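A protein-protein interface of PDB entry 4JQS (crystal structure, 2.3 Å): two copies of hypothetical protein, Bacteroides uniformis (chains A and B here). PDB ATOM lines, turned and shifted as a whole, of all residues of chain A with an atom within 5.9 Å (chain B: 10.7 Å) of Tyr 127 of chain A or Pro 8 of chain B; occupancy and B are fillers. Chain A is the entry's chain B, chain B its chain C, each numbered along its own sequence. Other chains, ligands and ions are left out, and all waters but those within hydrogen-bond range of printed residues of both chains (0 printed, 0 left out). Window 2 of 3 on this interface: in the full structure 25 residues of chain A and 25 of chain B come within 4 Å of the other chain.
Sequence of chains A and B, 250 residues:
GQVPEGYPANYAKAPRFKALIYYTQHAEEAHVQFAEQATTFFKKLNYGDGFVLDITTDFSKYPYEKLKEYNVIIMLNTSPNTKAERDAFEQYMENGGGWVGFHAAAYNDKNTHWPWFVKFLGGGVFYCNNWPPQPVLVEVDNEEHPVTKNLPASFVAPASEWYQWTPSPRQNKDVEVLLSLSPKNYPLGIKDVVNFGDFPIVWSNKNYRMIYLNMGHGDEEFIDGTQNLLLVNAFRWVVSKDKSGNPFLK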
ATOM      1  N   VAL A 125      26.005 -22.799 -40.600  1.00  0.00           N
ATOM      2  CA  VAL A 125      25.089 -23.923 -40.830  1.00  0.00           C
ATOM      3  C   VAL A 125      24.481 -24.275 -39.459  1.00  0.00           C
ATOM      4  O   VAL A 125      25.223 -24.217 -38.471  1.00  0.00           O
ATOM      5  CB  VAL A 125      25.815 -25.138 -41.479  1.00  0.00           C
ATOM      6  CG1 VAL A 125      24.842 -26.279 -41.770  1.00  0.00           C
ATOM      7  CG2 VAL A 125      26.558 -24.723 -42.750  1.00  0.00           C
ATOM      8  N   PHE A 126      23.163 -24.623 -39.381  1.00  0.00           N
ATOM      9  CA  PHE A 126      22.508 -24.990 -38.101  1.00  0.00           C
ATOM     10  C   PHE A 126      23.333 -26.037 -37.339  1.00  0.00           C
ATOM     11  O   PHE A 126      23.765 -27.032 -37.926  1.00  0.00           O
ATOM     12  CB  PHE A 126      21.069 -25.493 -38.297  1.00  0.00           C
ATOM     13  CG  PHE A 126      20.434 -25.890 -36.985  1.00  0.00           C
ATOM     14  CD1 PHE A 126      19.911 -24.928 -36.129  1.00  0.00           C
ATOM     15  CD2 PHE A 126      20.387 -27.225 -36.590  1.00  0.00           C
ATOM     16  CE1 PHE A 126      19.358 -25.289 -34.899  1.00  0.00           C
ATOM     17  CE2 PHE A 126      19.842 -27.585 -35.357  1.00  0.00           C
ATOM     18  CZ  PHE A 126      19.322 -26.613 -34.522  1.00  0.00           C
ATOM     19  N   TYR A 127      23.562 -25.794 -36.040  1.00  0.00           N
ATOM     20  CA  TYR A 127      24.396 -26.669 -35.224  1.00  0.00           C
ATOM     21  C   TYR A 127      23.596 -27.326 -34.091  1.00  0.00           C
ATOM     22  O   TYR A 127      23.555 -28.557 -34.007  1.00  0.00           O
ATOM     23  CB  TYR A 127      25.563 -25.847 -34.670  1.00  0.00           C
ATOM     24  CG  TYR A 127      26.665 -26.632 -34.012  1.00  0.00           C
ATOM     25  CD1 TYR A 127      27.135 -27.817 -34.573  1.00  0.00           C
ATOM     26  CD2 TYR A 127      27.326 -26.133 -32.891  1.00  0.00           C
ATOM     27  CE1 TYR A 127      28.198 -28.515 -34.004  1.00  0.00           C
ATOM     28  CE2 TYR A 127      28.415 -26.802 -32.336  1.00  0.00           C
ATOM     29  CZ  TYR A 127      28.835 -28.004 -32.888  1.00  0.00           C
ATOM     30  OH  TYR A 127      29.884 -28.692 -32.342  1.00  0.00           O
ATOM     31  N   CYS A 128      22.982 -26.508 -33.214  1.00  0.00           N
ATOM     32  CA  CYS A 128      22.161 -26.980 -32.097  1.00  0.00           C
ATOM     33  C   CYS A 128      21.211 -25.883 -31.608  1.00  0.00           C
ATOM     34  O   CYS A 128      21.206 -24.748 -32.107  1.00  0.00           O
ATOM     35  CB  CYS A 128      23.013 -27.533 -30.955  1.00  0.00           C
ATOM     36  SG  CYS A 128      23.904 -26.280 -30.005  1.00  0.00           S
ATOM     37  N   ASN A 129      20.382 -26.261 -30.639  1.00  0.00           N
ATOM     38  CA  ASN A 129      19.387 -25.399 -30.036  1.00  0.00           C
ATOM     39  C   ASN A 129      19.052 -25.882 -28.636  1.00  0.00           C
ATOM     40  O   ASN A 129      19.298 -27.052 -28.300  1.00  0.00           O
ATOM     41  CB  ASN A 129      18.105 -25.374 -30.903  1.00  0.00           C
ATOM     42  CG  ASN A 129      17.406 -26.718 -30.947  1.00  0.00           C
ATOM     43  OD1 ASN A 129      17.825 -27.628 -31.667  1.00  0.00           O
ATOM     44  ND2 ASN A 129      16.376 -26.902 -30.121  1.00  0.00           N
ATOM     45  N   GLN A 164      22.389 -22.196 -32.284  1.00  0.00           N
ATOM     46  CA  GLN A 164      23.829 -22.084 -32.464  1.00  0.00           C
ATOM     47  C   GLN A 164      24.128 -22.525 -33.894  1.00  0.00           C
ATOM     48  O   GLN A 164      23.381 -23.342 -34.473  1.00  0.00           O
ATOM     49  CB  GLN A 164      24.620 -22.915 -31.459  1.00  0.00           C
ATOM     50  CG  GLN A 164      24.936 -22.188 -30.163  1.00  0.00           C
ATOM     51  CD  GLN A 164      25.945 -22.936 -29.342  1.00  0.00           C
ATOM     52  OE1 GLN A 164      26.478 -23.974 -29.747  1.00  0.00           O
ATOM     53  NE2 GLN A 164      26.263 -22.408 -28.190  1.00  0.00           N
ATOM     54  N   TRP A 165      25.214 -21.985 -34.465  1.00  0.00           N
ATOM     55  CA  TRP A 165      25.602 -22.299 -35.840  1.00  0.00           C
ATOM     56  C   TRP A 165      27.035 -22.753 -35.881  1.00  0.00           C
ATOM     57  O   TRP A 165      27.805 -22.465 -34.963  1.00  0.00           O
ATOM     58  CB  TRP A 165      25.400 -21.085 -36.766  1.00  0.00           C
ATOM     59  CG  TRP A 165      24.107 -20.362 -36.535  1.00  0.00           C
ATOM     60  CD1 TRP A 165      23.857 -19.409 -35.588  1.00  0.00           C
ATOM     61  CD2 TRP A 165      22.881 -20.538 -37.266  1.00  0.00           C
ATOM     62  NE1 TRP A 165      22.562 -18.955 -35.702  1.00  0.00           N
ATOM     63  CE2 TRP A 165      21.929 -19.649 -36.709  1.00  0.00           C
ATOM     64  CE3 TRP A 165      22.508 -21.321 -38.377  1.00  0.00           C
ATOM     65  CZ2 TRP A 165      20.627 -19.530 -37.216  1.00  0.00           C
ATOM     66  CZ3 TRP A 165      21.205 -21.230 -38.853  1.00  0.00           C
ATOM     67  CH2 TRP A 165      20.280 -20.343 -38.274  1.00  0.00           C
ATOM     68  N   THR A 166      27.395 -23.463 -36.954  1.00  0.00           N
ATOM     69  CA  THR A 166      28.744 -23.929 -37.170  1.00  0.00           C
ATOM     70  C   THR A 166      29.120 -23.597 -38.619  1.00  0.00           C
ATOM     71  O   THR A 166      28.457 -24.071 -39.538  1.00  0.00           O
ATOM     72  CB  THR A 166      28.933 -25.409 -36.760  1.00  0.00           C
ATOM     73  OG1 THR A 166      30.330 -25.693 -36.710  1.00  0.00           O
ATOM     74  CG2 THR A 166      28.203 -26.415 -37.676  1.00  0.00           C
ATOM     75  N   VAL A 193      19.701 -29.341 -23.718  1.00  0.00           N
ATOM     76  CA  VAL A 193      20.631 -28.486 -22.983  1.00  0.00           C
ATOM     77  C   VAL A 193      21.869 -28.122 -23.816  1.00  0.00           C
ATOM     78  O   VAL A 193      22.578 -29.009 -24.289  1.00  0.00           O
ATOM     79  CB  VAL A 193      21.053 -29.190 -21.651  1.00  0.00           C
ATOM     80  CG1 VAL A 193      21.879 -28.265 -20.762  1.00  0.00           C
ATOM     81  CG2 VAL A 193      19.833 -29.722 -20.888  1.00  0.00           C
ATOM     82  N   VAL A 194      22.130 -26.808 -23.956  1.00  0.00           N
ATOM     83  CA  VAL A 194      23.325 -26.245 -24.612  1.00  0.00           C
ATOM     84  C   VAL A 194      24.249 -25.853 -23.440  1.00  0.00           C
ATOM     85  O   VAL A 194      23.837 -25.111 -22.541  1.00  0.00           O
ATOM     86  CB  VAL A 194      23.008 -25.081 -25.594  1.00  0.00           C
ATOM     87  CG1 VAL A 194      24.274 -24.595 -26.294  1.00  0.00           C
ATOM     88  CG2 VAL A 194      21.953 -25.496 -26.621  1.00  0.00           C
ATOM     89  N   ASN A 195      25.453 -26.432 -23.415  1.00  0.00           N
ATOM     90  CA  ASN A 195      26.416 -26.308 -22.329  1.00  0.00           C
ATOM     91  C   ASN A 195      27.538 -25.290 -22.549  1.00  0.00           C
ATOM     92  O   ASN A 195      28.138 -24.857 -21.565  1.00  0.00           O
ATOM     93  CB  ASN A 195      27.031 -27.687 -22.051  1.00  0.00           C
ATOM     94  CG  ASN A 195      26.001 -28.678 -21.532  1.00  0.00           C
ATOM     95  OD1 ASN A 195      25.365 -28.465 -20.485  1.00  0.00           O
ATOM     96  ND2 ASN A 195      25.759 -29.746 -22.295  1.00  0.00           N
ATOM     97  N   PHE A 196      27.845 -24.915 -23.804  1.00  0.00           N
ATOM     98  CA  PHE A 196      28.924 -23.963 -24.083  1.00  0.00           C
ATOM     99  C   PHE A 196      28.884 -23.486 -25.525  1.00  0.00           C
ATOM    100  O   PHE A 196      28.085 -23.968 -26.336  1.00  0.00           O
ATOM    101  CB  PHE A 196      30.308 -24.588 -23.771  1.00  0.00           C
ATOM    102  CG  PHE A 196      30.596 -25.853 -24.539  1.00  0.00           C
ATOM    103  CD1 PHE A 196      31.060 -25.799 -25.855  1.00  0.00           C
ATOM    104  CD2 PHE A 196      30.445 -27.103 -23.935  1.00  0.00           C
ATOM    105  CE1 PHE A 196      31.331 -26.971 -26.565  1.00  0.00           C
ATOM    106  CE2 PHE A 196      30.723 -28.278 -24.642  1.00  0.00           C
ATOM    107  CZ  PHE A 196      31.179 -28.204 -25.948  1.00  0.00           C
ATOM    108  N   GLY A 197      29.817 -22.602 -25.846  1.00  0.00           N
ATOM    109  CA  GLY A 197      29.998 -22.066 -27.182  1.00  0.00           C
ATOM    110  C   GLY A 197      29.524 -20.635 -27.333  1.00  0.00           C
ATOM    111  O   GLY A 197      28.770 -20.105 -26.502  1.00  0.00           O
ATOM    112  N   GLY B   6      33.477 -31.753 -27.021  1.00  0.00           N
ATOM    113  CA  GLY B   6      33.091 -31.808 -28.430  1.00  0.00           C
ATOM    114  C   GLY B   6      31.828 -31.020 -28.739  1.00  0.00           C
ATOM    115  O   GLY B   6      31.859 -29.786 -28.774  1.00  0.00           O
ATOM    116  N   TYR B   7      30.706 -31.735 -28.963  1.00  0.00           N
ATOM    117  CA  TYR B   7      29.393 -31.160 -29.269  1.00  0.00           C
ATOM    118  C   TYR B   7      28.816 -30.477 -28.011  1.00  0.00           C
ATOM    119  O   TYR B   7      28.837 -31.078 -26.933  1.00  0.00           O
ATOM    120  CB  TYR B   7      28.464 -32.257 -29.796  1.00  0.00           C
ATOM    121  CG  TYR B   7      27.144 -31.769 -30.352  1.00  0.00           C
ATOM    122  CD1 TYR B   7      27.097 -30.960 -31.485  1.00  0.00           C
ATOM    123  CD2 TYR B   7      25.938 -32.198 -29.807  1.00  0.00           C
ATOM    124  CE1 TYR B   7      25.881 -30.530 -32.016  1.00  0.00           C
ATOM    125  CE2 TYR B   7      24.718 -31.788 -30.339  1.00  0.00           C
ATOM    126  CZ  TYR B   7      24.692 -30.956 -31.445  1.00  0.00           C
ATOM    127  OH  TYR B   7      23.480 -30.591 -31.980  1.00  0.00           O
ATOM    128  N   PRO B   8      28.341 -29.212 -28.115  1.00  0.00           N
ATOM    129  CA  PRO B   8      27.873 -28.501 -26.911  1.00  0.00           C
ATOM    130  C   PRO B   8      26.469 -28.842 -26.405  1.00  0.00           C
ATOM    131  O   PRO B   8      26.123 -28.381 -25.309  1.00  0.00           O
ATOM    132  CB  PRO B   8      27.917 -27.026 -27.335  1.00  0.00           C
ATOM    133  CG  PRO B   8      27.830 -27.026 -28.794  1.00  0.00           C
ATOM    134  CD  PRO B   8      28.304 -28.342 -29.310  1.00  0.00           C
ATOM    135  N   ALA B   9      25.664 -29.610 -27.176  1.00  0.00           N
ATOM    136  CA  ALA B   9      24.279 -29.871 -26.787  1.00  0.00           C
ATOM    137  C   ALA B   9      23.966 -31.322 -26.408  1.00  0.00           C
ATOM    138  O   ALA B   9      24.416 -32.277 -27.051  1.00  0.00           O
ATOM    139  CB  ALA B   9      23.324 -29.413 -27.887  1.00  0.00           C
ATOM    140  N   ASN B  10      23.127 -31.448 -25.363  1.00  0.00           N
ATOM    141  CA  ASN B  10      22.618 -32.690 -24.806  1.00  0.00           C
ATOM    142  C   ASN B  10      21.103 -32.752 -25.064  1.00  0.00           C
ATOM    143  O   ASN B  10      20.311 -32.123 -24.347  1.00  0.00           O
ATOM    144  CB  ASN B  10      22.953 -32.792 -23.297  1.00  0.00           C
ATOM    145  CG  ASN B  10      22.487 -34.056 -22.587  1.00  0.00           C
ATOM    146  OD1 ASN B  10      21.829 -34.955 -23.141  1.00  0.00           O
ATOM    147  ND2 ASN B  10      22.804 -34.137 -21.307  1.00  0.00           N
ATOM    148  N   TYR B  11      20.720 -33.506 -26.110  1.00  0.00           N
ATOM    149  CA  TYR B  11      19.327 -33.729 -26.505  1.00  0.00           C
ATOM    150  C   TYR B  11      18.735 -34.896 -25.698  1.00  0.00           C
ATOM    151  O   TYR B  11      19.319 -35.981 -25.683  1.00  0.00           O
ATOM    152  CB  TYR B  11      19.232 -33.990 -28.029  1.00  0.00           C
ATOM    153  CG  TYR B  11      19.423 -32.739 -28.865  1.00  0.00           C
ATOM    154  CD1 TYR B  11      20.693 -32.345 -29.289  1.00  0.00           C
ATOM    155  CD2 TYR B  11      18.332 -31.970 -29.267  1.00  0.00           C
ATOM    156  CE1 TYR B  11      20.873 -31.201 -30.069  1.00  0.00           C
ATOM    157  CE2 TYR B  11      18.502 -30.819 -30.042  1.00  0.00           C
ATOM    158  CZ  TYR B  11      19.775 -30.434 -30.432  1.00  0.00           C
ATOM    159  OH  TYR B  11      19.934 -29.316 -31.217  1.00  0.00           O
ATOM    160  N   ALA B  12      17.601 -34.666 -25.000  1.00  0.00           N
ATOM    161  CA  ALA B  12      16.955 -35.727 -24.207  1.00  0.00           C
ATOM    162  C   ALA B  12      16.475 -36.891 -25.109  1.00  0.00           C
ATOM    163  O   ALA B  12      15.969 -36.665 -26.208  1.00  0.00           O
ATOM    164  CB  ALA B  12      15.791 -35.175 -23.400  1.00  0.00           C
ATOM    165  N   ARG B  16      13.184 -36.514 -18.709  1.00  0.00           N
ATOM    166  CA  ARG B  16      14.312 -36.502 -17.767  1.00  0.00           C
ATOM    167  C   ARG B  16      13.944 -36.747 -16.296  1.00  0.00           C
ATOM    168  O   ARG B  16      14.775 -37.257 -15.542  1.00  0.00           O
ATOM    169  CB  ARG B  16      15.054 -35.163 -17.862  1.00  0.00           C
ATOM    170  CG  ARG B  16      15.756 -34.912 -19.184  1.00  0.00           C
ATOM    171  CD  ARG B  16      16.593 -33.630 -19.142  1.00  0.00           C
ATOM    172  NE  ARG B  16      17.328 -33.422 -20.401  1.00  0.00           N
ATOM    173  CZ  ARG B  16      18.503 -33.980 -20.683  1.00  0.00           C
ATOM    174  NH1 ARG B  16      19.094 -34.778 -19.803  1.00  0.00           N
ATOM    175  NH2 ARG B  16      19.084 -33.759 -21.854  1.00  0.00           N
ATOM    176  N   ARG B 236      14.449 -25.217 -12.420  1.00  0.00           N
ATOM    177  CA  ARG B 236      15.627 -25.928 -12.928  1.00  0.00           C
ATOM    178  C   ARG B 236      16.636 -26.255 -11.811  1.00  0.00           C
ATOM    179  O   ARG B 236      17.167 -27.364 -11.779  1.00  0.00           O
ATOM    180  CB  ARG B 236      16.311 -25.101 -14.036  1.00  0.00           C
ATOM    181  CG  ARG B 236      17.312 -25.888 -14.844  1.00  0.00           C
ATOM    182  CD  ARG B 236      18.127 -25.016 -15.793  1.00  0.00           C
ATOM    183  NE  ARG B 236      18.717 -25.832 -16.861  1.00  0.00           N
ATOM    184  CZ  ARG B 236      19.770 -26.637 -16.725  1.00  0.00           C
ATOM    185  NH1 ARG B 236      20.404 -26.724 -15.560  1.00  0.00           N
ATOM    186  NH2 ARG B 236      20.185 -27.375 -17.746  1.00  0.00           N
ATOM    187  N   PHE B 248      19.615 -33.326 -15.862  1.00  0.00           N
ATOM    188  CA  PHE B 248      20.036 -32.629 -17.076  1.00  0.00           C
ATOM    189  C   PHE B 248      21.369 -33.143 -17.639  1.00  0.00           C
ATOM    190  O   PHE B 248      21.765 -32.692 -18.706  1.00  0.00           O
ATOM    191  CB  PHE B 248      20.092 -31.117 -16.822  1.00  0.00           C
ATOM    192  CG  PHE B 248      18.767 -30.593 -16.321  1.00  0.00           C
ATOM    193  CD1 PHE B 248      17.630 -30.646 -17.125  1.00  0.00           C
ATOM    194  CD2 PHE B 248      18.648 -30.068 -15.036  1.00  0.00           C
ATOM    195  CE1 PHE B 248      16.401 -30.199 -16.653  1.00  0.00           C
ATOM    196  CE2 PHE B 248      17.426 -29.591 -14.576  1.00  0.00           C
ATOM    197  CZ  PHE B 248      16.311 -29.646 -15.394  1.00  0.00           C
ATOM    198  N   LEU B 249      22.030 -34.105 -16.960  1.00  0.00           N
ATOM    199  CA  LEU B 249      23.301 -34.687 -17.411  1.00  0.00           C
ATOM    200  C   LEU B 249      23.083 -36.045 -18.082  1.00  0.00           C
ATOM    201  O   LEU B 249      24.029 -36.609 -18.624  1.00  0.00           O
ATOM    202  CB  LEU B 249      24.317 -34.816 -16.251  1.00  0.00           C
ATOM    203  CG  LEU B 249      24.540 -33.576 -15.373  1.00  0.00           C
ATOM    204  CD1 LEU B 249      25.587 -33.853 -14.303  1.00  0.00           C
ATOM    205  CD2 LEU B 249      24.930 -32.339 -16.202  1.00  0.00           C
ATOM    206  N   LYS B 250      21.837 -36.560 -18.065  1.00  0.00           N
ATOM    207  CA  LYS B 250      21.476 -37.843 -18.688  1.00  0.00           C
ATOM    208  C   LYS B 250      21.520 -37.768 -20.227  1.00  0.00           C
ATOM    209  O   LYS B 250      21.295 -36.671 -20.785  1.00  0.00           O
ATOM    210  CB  LYS B 250      20.070 -38.299 -18.238  1.00  0.00           C
ATOM    211  CG  LYS B 250      19.930 -38.499 -16.730  1.00  0.00           C
ATOM    212  CD  LYS B 250      18.778 -39.418 -16.349  1.00  0.00           C
ATOM    213  CE  LYS B 250      17.426 -38.796 -16.570  1.00  0.00           C
ATOM    214  NZ  LYS B 250      16.330 -39.625 -16.008  1.00  0.00           N
ATOM    215  OXT LYS B 250      21.748 -38.818 -20.872  1.00  0.00           O
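N of Tyr 127 of chain A sits at hydrogen-bond distance from O of Gln 164 of chain A, 2.9 Å away.
The backbone NH (N) of Gln 164 of chain A lies within hydrogen-bond range of the backbone carbonyl oxygen (O) of Cys 128 of chain A (2.8 Å).
NE2 of Gln 164 of chain A sits at hydrogen-bond distance from O of Phe 196 of chain A (3.0 Å).
The backbone carbonyl oxygen (O) of Asn 10 of chain B lies within hydrogen-bond range of the guanidinium group (NH2) of Arg 16 of chain B (3.2 Å).
ND2 of Asn 10 of chain B is in hydrogen-bond range of O of Phe 248 of chain B, at 3.2 Å.
The chain-end carboxylate of Lys 250 of chain B lies close to the side-chain amide oxygen of Asn 10 of chain B.
The backbone carbonyl oxygen (O) of Tyr 127 of chain A lies within hydrogen-bond range of the side-chain hydroxyl (OH) of Tyr 7 of chain B (2.9 Å).
The side-chain amide oxygen of Asn 129 of chain A is in hydrogen-bond range of the side-chain hydroxyl of Tyr 11 of chain B (2.7 Å).
The backbone NH (N) of Asn 10 of chain B is in hydrogen-bond range of the backbone carbonyl oxygen (O) of Val 193 of chain A.
N of Asn 195 of chain A sits at hydrogen-bond distance from O of Pro 8 of chain B, 2.8 Å away.
Pro 8 of chain B touches Tyr 127 of chain A (CD to CE2, 3.4 Å).
Cys 128 of chain A touches Tyr 7 of chain B.
Ala 9 of chain B touches Cys 128 of chain A (CB to CB, 3.6 Å).
CA of Cys 128 of chain A touches OH of Tyr 11 of chain B (3.3 Å).
O of Val 193 of chain A touches O of Pro 8 of chain B (3.7 Å).
CA of Ala 9 of chain B touches O of Val 193 of chain A, at 3.1 Å.
Pro 8 of chain B touches Val 194 of chain A.
Phe 196 of chain A touches Gly 6 of chain B.
CZ of Phe 196 of chain A touches O of Tyr 7 of chain B, 3.8 Å away.
CB of Pro 8 of chain B touches O of Phe 196 of chain A, at 3.2 Å.
No residue of chain B comes within 4 Å of Phe 126 of chain A.
Of chain B, only Tyr 7 and Pro 8 come within 4 Å of Tyr 127 of chain A.
Of chain B, only Tyr 7 (3.3 Å), Ala 9 (3.6 Å) and Tyr 11 (3.3 Å) come within 4 Å of Cys 128 of chain A.
No residue of chain B comes within 4 Å of Thr 166 of chain A.
Of chain B, only Pro 8 (3.6 Å) comes within 4 Å of Val 194 of chain A.
Of chain B, only Pro 8 comes within 4 Å of Asn 195 of chain A.
Printed residues of chain A within 4 Å of Gly 6 of chain B: Phe 196.
Of chain A, only Tyr 127, Gln 164, Val 193, Val 194, Asn 195 and Phe 196 come within 4 Å of Pro 8 of chain B.
Printed residues of chain A within 4 Å of Arg 236 of chain B: Val 193.
The nearest printed residue of chain A that does not touch Gly 6 of chain B is Tyr 127 of chain A (4.2 Å).
Printed residues of chain A that touch a printed residue of chain B: Tyr 127, Cys 128, Asn 129, Gln 164, Val 193, Val 194, Asn 195 and Phe 196.
Of the 12 printed residues of chain B, 7 touch a printed residue of chain A.
Printed residues of chain B that touch a printed residue of chain A: Gly 6, Tyr 7, Pro 8, Ala 9, Asn 10, Tyr 11 and Arg 236.
Along chain B the printed residues that touch a printed residue of chain A span positions 6 to 236.
Among the printed residues, no Asp or Glu carboxylate lies within 4 Å of a Lys or Arg side-chain nitrogen of the other chain.
No position is printed for both chains.
Of the 16 pairs that touch across the chains among the printed residues, none has its exchanged pair printed and touching as well.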
